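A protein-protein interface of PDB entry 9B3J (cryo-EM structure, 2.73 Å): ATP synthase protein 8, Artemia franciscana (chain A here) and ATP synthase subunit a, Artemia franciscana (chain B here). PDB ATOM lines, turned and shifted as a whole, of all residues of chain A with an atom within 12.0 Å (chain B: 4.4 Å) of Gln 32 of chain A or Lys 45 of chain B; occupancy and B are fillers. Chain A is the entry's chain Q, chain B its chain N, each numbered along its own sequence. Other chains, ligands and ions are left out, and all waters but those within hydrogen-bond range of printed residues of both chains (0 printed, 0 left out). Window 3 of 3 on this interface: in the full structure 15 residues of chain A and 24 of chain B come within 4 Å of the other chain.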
ATOM      1  N   ILE A  23      10.131  24.889 -15.525  1.00  0.00           N
ATOM      2  CA  ILE A  23       9.601  25.021 -14.171  1.00  0.00           C
ATOM      3  C   ILE A  23       8.312  25.831 -14.187  1.00  0.00           C
ATOM      4  O   ILE A  23       7.365  25.541 -13.441  1.00  0.00           O
ATOM      5  CB  ILE A  23      10.664  25.634 -13.244  1.00  0.00           C
ATOM      6  CG1 ILE A  23      11.751  24.602 -12.978  1.00  0.00           C
ATOM      7  CG2 ILE A  23      10.066  26.104 -11.938  1.00  0.00           C
ATOM      8  CD1 ILE A  23      12.750  25.022 -11.954  1.00  0.00           C
ATOM      9  N   MET A  26       5.643  23.595 -15.195  1.00  0.00           N
ATOM     10  CA  MET A  26       5.319  22.609 -14.168  1.00  0.00           C
ATOM     11  C   MET A  26       4.434  23.210 -13.084  1.00  0.00           C
ATOM     12  O   MET A  26       3.524  22.543 -12.583  1.00  0.00           O
ATOM     13  CB  MET A  26       6.593  22.038 -13.541  1.00  0.00           C
ATOM     14  CG  MET A  26       7.399  21.093 -14.427  1.00  0.00           C
ATOM     15  SD  MET A  26       6.555  19.578 -14.900  1.00  0.00           S
ATOM     16  CE  MET A  26       6.961  18.511 -13.523  1.00  0.00           C
ATOM     17  N   VAL A  27       4.698  24.463 -12.705  1.00  0.00           N
ATOM     18  CA  VAL A  27       3.869  25.146 -11.714  1.00  0.00           C
ATOM     19  C   VAL A  27       2.491  25.458 -12.279  1.00  0.00           C
ATOM     20  O   VAL A  27       1.494  25.435 -11.547  1.00  0.00           O
ATOM     21  CB  VAL A  27       4.592  26.412 -11.221  1.00  0.00           C
ATOM     22  CG1 VAL A  27       3.759  27.177 -10.234  1.00  0.00           C
ATOM     23  CG2 VAL A  27       5.877  26.031 -10.561  1.00  0.00           C
ATOM     24  N   PHE A  28       2.403  25.726 -13.586  1.00  0.00           N
ATOM     25  CA  PHE A  28       1.132  26.103 -14.204  1.00  0.00           C
ATOM     26  C   PHE A  28       0.087  25.006 -14.079  1.00  0.00           C
ATOM     27  O   PHE A  28      -1.108  25.297 -14.012  1.00  0.00           O
ATOM     28  CB  PHE A  28       1.342  26.451 -15.677  1.00  0.00           C
ATOM     29  CG  PHE A  28       0.113  26.977 -16.358  1.00  0.00           C
ATOM     30  CD1 PHE A  28      -0.253  28.300 -16.228  1.00  0.00           C
ATOM     31  CD2 PHE A  28      -0.671  26.152 -17.141  1.00  0.00           C
ATOM     32  CE1 PHE A  28      -1.379  28.785 -16.857  1.00  0.00           C
ATOM     33  CE2 PHE A  28      -1.799  26.634 -17.769  1.00  0.00           C
ATOM     34  CZ  PHE A  28      -2.149  27.948 -17.628  1.00  0.00           C
ATOM     35  N   PHE A  29       0.504  23.752 -14.027  1.00  0.00           N
ATOM     36  CA  PHE A  29      -0.436  22.663 -13.853  1.00  0.00           C
ATOM     37  C   PHE A  29      -0.480  22.154 -12.427  1.00  0.00           C
ATOM     38  O   PHE A  29      -1.041  21.084 -12.182  1.00  0.00           O
ATOM     39  CB  PHE A  29      -0.101  21.525 -14.804  1.00  0.00           C
ATOM     40  CG  PHE A  29      -0.664  21.710 -16.169  1.00  0.00           C
ATOM     41  CD1 PHE A  29      -0.205  22.717 -16.986  1.00  0.00           C
ATOM     42  CD2 PHE A  29      -1.663  20.880 -16.630  1.00  0.00           C
ATOM     43  CE1 PHE A  29      -0.728  22.888 -18.227  1.00  0.00           C
ATOM     44  CE2 PHE A  29      -2.188  21.051 -17.874  1.00  0.00           C
ATOM     45  CZ  PHE A  29      -1.721  22.054 -18.672  1.00  0.00           C
ATOM     46  N   LEU A  30       0.102  22.887 -11.485  1.00  0.00           N
ATOM     47  CA  LEU A  30       0.093  22.503 -10.075  1.00  0.00           C
ATOM     48  C   LEU A  30      -1.009  23.297  -9.388  1.00  0.00           C
ATOM     49  O   LEU A  30      -0.772  24.361  -8.821  1.00  0.00           O
ATOM     50  CB  LEU A  30       1.445  22.753  -9.425  1.00  0.00           C
ATOM     51  CG  LEU A  30       1.614  22.132  -8.045  1.00  0.00           C
ATOM     52  CD1 LEU A  30       1.658  20.632  -8.184  1.00  0.00           C
ATOM     53  CD2 LEU A  30       2.858  22.643  -7.372  1.00  0.00           C
ATOM     54  N   TYR A  31      -2.227  22.772  -9.449  1.00  0.00           N
ATOM     55  CA  TYR A  31      -3.345  23.371  -8.740  1.00  0.00           C
ATOM     56  C   TYR A  31      -4.351  22.279  -8.421  1.00  0.00           C
ATOM     57  O   TYR A  31      -4.397  21.241  -9.085  1.00  0.00           O
ATOM     58  CB  TYR A  31      -3.997  24.486  -9.558  1.00  0.00           C
ATOM     59  CG  TYR A  31      -4.989  23.990 -10.576  1.00  0.00           C
ATOM     60  CD1 TYR A  31      -4.575  23.273 -11.688  1.00  0.00           C
ATOM     61  CD2 TYR A  31      -6.341  24.247 -10.428  1.00  0.00           C
ATOM     62  CE1 TYR A  31      -5.481  22.821 -12.617  1.00  0.00           C
ATOM     63  CE2 TYR A  31      -7.252  23.803 -11.351  1.00  0.00           C
ATOM     64  CZ  TYR A  31      -6.817  23.090 -12.442  1.00  0.00           C
ATOM     65  OH  TYR A  31      -7.728  22.647 -13.364  1.00  0.00           O
ATOM     66  N   GLN A  32      -5.162  22.522  -7.393  1.00  0.00           N
ATOM     67  CA  GLN A  32      -6.162  21.548  -6.989  1.00  0.00           C
ATOM     68  C   GLN A  32      -7.533  22.016  -7.436  1.00  0.00           C
ATOM     69  O   GLN A  32      -8.042  23.008  -6.896  1.00  0.00           O
ATOM     70  CB  GLN A  32      -6.145  21.334  -5.480  1.00  0.00           C
ATOM     71  CG  GLN A  32      -7.199  20.349  -5.006  1.00  0.00           C
ATOM     72  CD  GLN A  32      -7.001  18.953  -5.570  1.00  0.00           C
ATOM     73  OE1 GLN A  32      -5.876  18.518  -5.804  1.00  0.00           O
ATOM     74  NE2 GLN A  32      -8.099  18.242  -5.785  1.00  0.00           N
ATOM     75  N   PRO A  33      -8.164  21.350  -8.391  1.00  0.00           N
ATOM     76  CA  PRO A  33      -9.476  21.806  -8.857  1.00  0.00           C
ATOM     77  C   PRO A  33     -10.571  21.489  -7.857  1.00  0.00           C
ATOM     78  O   PRO A  33     -11.009  20.341  -7.740  1.00  0.00           O
ATOM     79  CB  PRO A  33      -9.660  21.042 -10.171  1.00  0.00           C
ATOM     80  CG  PRO A  33      -8.836  19.819 -10.014  1.00  0.00           C
ATOM     81  CD  PRO A  33      -7.676  20.183  -9.141  1.00  0.00           C
ATOM     82  N   ARG A  34     -11.032  22.505  -7.136  1.00  0.00           N
ATOM     83  CA  ARG A  34     -12.017  22.312  -6.081  1.00  0.00           C
ATOM     84  C   ARG A  34     -13.411  22.403  -6.685  1.00  0.00           C
ATOM     85  O   ARG A  34     -13.835  23.472  -7.135  1.00  0.00           O
ATOM     86  CB  ARG A  34     -11.827  23.337  -4.969  1.00  0.00           C
ATOM     87  CG  ARG A  34     -10.676  23.017  -4.044  1.00  0.00           C
ATOM     88  CD  ARG A  34     -10.741  23.863  -2.793  1.00  0.00           C
ATOM     89  NE  ARG A  34      -9.652  23.560  -1.873  1.00  0.00           N
ATOM     90  CZ  ARG A  34      -9.547  24.058  -0.649  1.00  0.00           C
ATOM     91  NH1 ARG A  34     -10.454  24.889  -0.161  1.00  0.00           N
ATOM     92  NH2 ARG A  34      -8.507  23.714   0.104  1.00  0.00           N
ATOM     93  N   SER A  35     -14.119  21.276  -6.698  1.00  0.00           N
ATOM     94  CA  SER A  35     -15.499  21.227  -7.176  1.00  0.00           C
ATOM     95  C   SER A  35     -16.450  21.456  -6.002  1.00  0.00           C
ATOM     96  O   SER A  35     -17.128  20.552  -5.515  1.00  0.00           O
ATOM     97  CB  SER A  35     -15.778  19.899  -7.864  1.00  0.00           C
ATOM     98  OG  SER A  35     -17.157  19.773  -8.151  1.00  0.00           O
ATOM     99  N   VAL A  36     -16.491  22.708  -5.552  1.00  0.00           N
ATOM    100  CA  VAL A  36     -17.355  23.091  -4.441  1.00  0.00           C
ATOM    101  C   VAL A  36     -18.476  23.961  -4.993  1.00  0.00           C
ATOM    102  O   VAL A  36     -18.986  24.857  -4.310  1.00  0.00           O
ATOM    103  CB  VAL A  36     -16.571  23.815  -3.330  1.00  0.00           C
ATOM    104  CG1 VAL A  36     -17.199  23.545  -1.966  1.00  0.00           C
ATOM    105  CG2 VAL A  36     -15.121  23.380  -3.330  1.00  0.00           C
ATOM    106  N   SER A  37     -18.854  23.714  -6.243  1.00  0.00           N
ATOM    107  CA  SER A  37     -19.962  24.431  -6.867  1.00  0.00           C
ATOM    108  C   SER A  37     -21.269  23.905  -6.290  1.00  0.00           C
ATOM    109  O   SER A  37     -21.793  22.882  -6.734  1.00  0.00           O
ATOM    110  CB  SER A  37     -19.919  24.263  -8.381  1.00  0.00           C
ATOM    111  OG  SER A  37     -20.983  24.968  -8.997  1.00  0.00           O
ATOM    112  N   LEU B  35      -6.803  12.863  -7.944  1.00  0.00           N
ATOM    113  CA  LEU B  35      -7.572  14.085  -7.738  1.00  0.00           C
ATOM    114  C   LEU B  35      -7.304  14.677  -6.365  1.00  0.00           C
ATOM    115  O   LEU B  35      -7.075  15.883  -6.232  1.00  0.00           O
ATOM    116  CB  LEU B  35      -9.059  13.805  -7.920  1.00  0.00           C
ATOM    117  CG  LEU B  35      -9.988  14.976  -7.634  1.00  0.00           C
ATOM    118  CD1 LEU B  35      -9.718  16.118  -8.583  1.00  0.00           C
ATOM    119  CD2 LEU B  35     -11.412  14.511  -7.756  1.00  0.00           C
ATOM    120  N   PRO B  37      -4.738  15.209  -3.568  1.00  0.00           N
ATOM    121  CA  PRO B  37      -3.278  15.184  -3.694  1.00  0.00           C
ATOM    122  C   PRO B  37      -2.628  14.338  -2.612  1.00  0.00           C
ATOM    123  O   PRO B  37      -3.248  13.949  -1.625  1.00  0.00           O
ATOM    124  CB  PRO B  37      -2.886  16.657  -3.568  1.00  0.00           C
ATOM    125  CG  PRO B  37      -4.018  17.311  -2.898  1.00  0.00           C
ATOM    126  CD  PRO B  37      -5.249  16.533  -3.192  1.00  0.00           C
ATOM    127  N   GLN B  41       2.710  16.792  -2.761  1.00  0.00           N
ATOM    128  CA  GLN B  41       2.038  17.680  -3.698  1.00  0.00           C
ATOM    129  C   GLN B  41       1.240  18.743  -2.966  1.00  0.00           C
ATOM    130  O   GLN B  41       1.268  19.918  -3.344  1.00  0.00           O
ATOM    131  CB  GLN B  41       1.127  16.878  -4.616  1.00  0.00           C
ATOM    132  CG  GLN B  41       0.349  17.732  -5.578  1.00  0.00           C
ATOM    133  CD  GLN B  41      -0.696  16.949  -6.322  1.00  0.00           C
ATOM    134  OE1 GLN B  41      -0.667  15.719  -6.357  1.00  0.00           O
ATOM    135  NE2 GLN B  41      -1.646  17.659  -6.910  1.00  0.00           N
ATOM    136  N   PHE B  42       0.534  18.353  -1.906  1.00  0.00           N
ATOM    137  CA  PHE B  42      -0.222  19.327  -1.132  1.00  0.00           C
ATOM    138  C   PHE B  42       0.700  20.309  -0.430  1.00  0.00           C
ATOM    139  O   PHE B  42       0.397  21.502  -0.359  1.00  0.00           O
ATOM    140  CB  PHE B  42      -1.120  18.633  -0.116  1.00  0.00           C
ATOM    141  CG  PHE B  42      -1.840  19.584   0.787  1.00  0.00           C
ATOM    142  CD1 PHE B  42      -2.908  20.318   0.318  1.00  0.00           C
ATOM    143  CD2 PHE B  42      -1.439  19.762   2.099  1.00  0.00           C
ATOM    144  CE1 PHE B  42      -3.568  21.205   1.137  1.00  0.00           C
ATOM    145  CE2 PHE B  42      -2.093  20.649   2.922  1.00  0.00           C
ATOM    146  CZ  PHE B  42      -3.160  21.369   2.440  1.00  0.00           C
ATOM    147  N   LEU B  43       1.828  19.827   0.097  1.00  0.00           N
ATOM    148  CA  LEU B  43       2.759  20.727   0.771  1.00  0.00           C
ATOM    149  C   LEU B  43       3.401  21.704  -0.206  1.00  0.00           C
ATOM    150  O   LEU B  43       3.546  22.897   0.100  1.00  0.00           O
ATOM    151  CB  LEU B  43       3.824  19.916   1.497  1.00  0.00           C
ATOM    152  CG  LEU B  43       3.362  19.249   2.783  1.00  0.00           C
ATOM    153  CD1 LEU B  43       4.324  18.143   3.139  1.00  0.00           C
ATOM    154  CD2 LEU B  43       3.276  20.270   3.891  1.00  0.00           C
ATOM    155  N   ALA B  44       3.777  21.221  -1.392  1.00  0.00           N
ATOM    156  CA  ALA B  44       4.344  22.101  -2.404  1.00  0.00           C
ATOM    157  C   ALA B  44       3.322  23.120  -2.883  1.00  0.00           C
ATOM    158  O   ALA B  44       3.643  24.307  -3.031  1.00  0.00           O
ATOM    159  CB  ALA B  44       4.874  21.280  -3.575  1.00  0.00           C
ATOM    160  N   LYS B  45       2.078  22.687  -3.101  1.00  0.00           N
ATOM    161  CA  LYS B  45       1.053  23.617  -3.547  1.00  0.00           C
ATOM    162  C   LYS B  45       0.698  24.623  -2.464  1.00  0.00           C
ATOM    163  O   LYS B  45       0.412  25.779  -2.773  1.00  0.00           O
ATOM    164  CB  LYS B  45      -0.198  22.866  -3.990  1.00  0.00           C
ATOM    165  CG  LYS B  45      -1.097  23.711  -4.859  1.00  0.00           C
ATOM    166  CD  LYS B  45      -2.555  23.501  -4.542  1.00  0.00           C
ATOM    167  CE  LYS B  45      -3.401  24.569  -5.213  1.00  0.00           C
ATOM    168  NZ  LYS B  45      -4.847  24.385  -4.917  1.00  0.00           N
ATOM    169  N   SER B  46       0.722  24.212  -1.197  1.00  0.00           N
ATOM    170  CA  SER B  46       0.421  25.136  -0.112  1.00  0.00           C
ATOM    171  C   SER B  46       1.496  26.199   0.029  1.00  0.00           C
ATOM    172  O   SER B  46       1.185  27.370   0.278  1.00  0.00           O
ATOM    173  CB  SER B  46       0.261  24.369   1.193  1.00  0.00           C
ATOM    174  OG  SER B  46      -0.744  23.382   1.073  1.00  0.00           O
ATOM    175  N   VAL B  47       2.767  25.816  -0.129  1.00  0.00           N
ATOM    176  CA  VAL B  47       3.837  26.809  -0.071  1.00  0.00           C
ATOM    177  C   VAL B  47       3.752  27.765  -1.256  1.00  0.00           C
ATOM    178  O   VAL B  47       3.907  28.987  -1.103  1.00  0.00           O
ATOM    179  CB  VAL B  47       5.206  26.111   0.003  1.00  0.00           C
ATOM    180  CG1 VAL B  47       6.325  27.124  -0.090  1.00  0.00           C
ATOM    181  CG2 VAL B  47       5.325  25.343   1.295  1.00  0.00           C
ATOM    182  N   LEU B  48       3.484  27.232  -2.452  1.00  0.00           N
ATOM    183  CA  LEU B  48       3.357  28.084  -3.629  1.00  0.00           C
ATOM    184  C   LEU B  48       2.158  29.016  -3.532  1.00  0.00           C
ATOM    185  O   LEU B  48       2.243  30.179  -3.931  1.00  0.00           O
ATOM    186  CB  LEU B  48       3.261  27.228  -4.883  1.00  0.00           C
ATOM    187  CG  LEU B  48       4.549  26.520  -5.278  1.00  0.00           C
ATOM    188  CD1 LEU B  48       4.408  25.945  -6.666  1.00  0.00           C
ATOM    189  CD2 LEU B  48       5.718  27.476  -5.208  1.00  0.00           C
ATOM    190  N   MET B  49       1.032  28.528  -3.013  1.00  0.00           N
ATOM    191  CA  MET B  49      -0.132  29.386  -2.842  1.00  0.00           C
ATOM    192  C   MET B  49       0.125  30.462  -1.801  1.00  0.00           C
ATOM    193  O   MET B  49      -0.327  31.602  -1.961  1.00  0.00           O
ATOM    194  CB  MET B  49      -1.354  28.558  -2.458  1.00  0.00           C
ATOM    195  CG  MET B  49      -1.964  27.808  -3.614  1.00  0.00           C
ATOM    196  SD  MET B  49      -2.174  28.877  -5.042  1.00  0.00           S
ATOM    197  CE  MET B  49      -3.411  30.026  -4.445  1.00  0.00           C
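Lys 45 of chain B touches two residues of chain A.
Of chain A, only Gln 32 (2.6 Å) comes within 4 Å of Leu 35 of chain B.
No residue of chain A comes within 4 Å of Phe 42 of chain B.
No residue of chain A comes within 4 Å of Ala 44 of chain B.
No residue of chain A comes within 4 Å of Val 47 of chain B.
Met 49 of chain B touches none of the printed residues of chain A.
Printed residues of chain B within 4 Å of Val 27 of chain A: Leu 48.
Printed residues of chain B within 4 Å of Leu 30 of chain A: Leu 48.
Of the printed residues of chain B, Tyr 31 of chain A touches Lys 45.
Pro 33 of chain A touches none of the printed residues of chain B.
The nearest printed residue of chain B that does not touch Gln 32 of chain A is Gln 41 of chain B (4.5 Å).
The nearest residue of chain A that does not touch Lys 45 of chain B is Leu 30 of chain A (4.03 Å).
The backbone carbonyl oxygen (O) of Leu 35 of chain B sits at hydrogen-bond distance from the side-chain amide nitrogen (NE2) of Gln 32 of chain A, at 2.6 Å.
The side-chain amino group (NZ) of Lys 45 of chain B sits close to the backbone NH (N) of Gln 32 of chain A (3.1 Å).
Hydrophobic or aromatic side chains of chain A within 4 Å of the printed part of chain B: Val 27 and Leu 30.
Among the printed residues, 6 pairs touch across the chains.
Among the printed residues, pairs that only touch across the chains: Gln 32 of chain A with Pro 37 of chain B, Leu 30 of chain A with Leu 48 of chain B, Tyr 31 of chain A with Lys 45 of chain B and Val 27 of chain A with Leu 48 of chain B.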
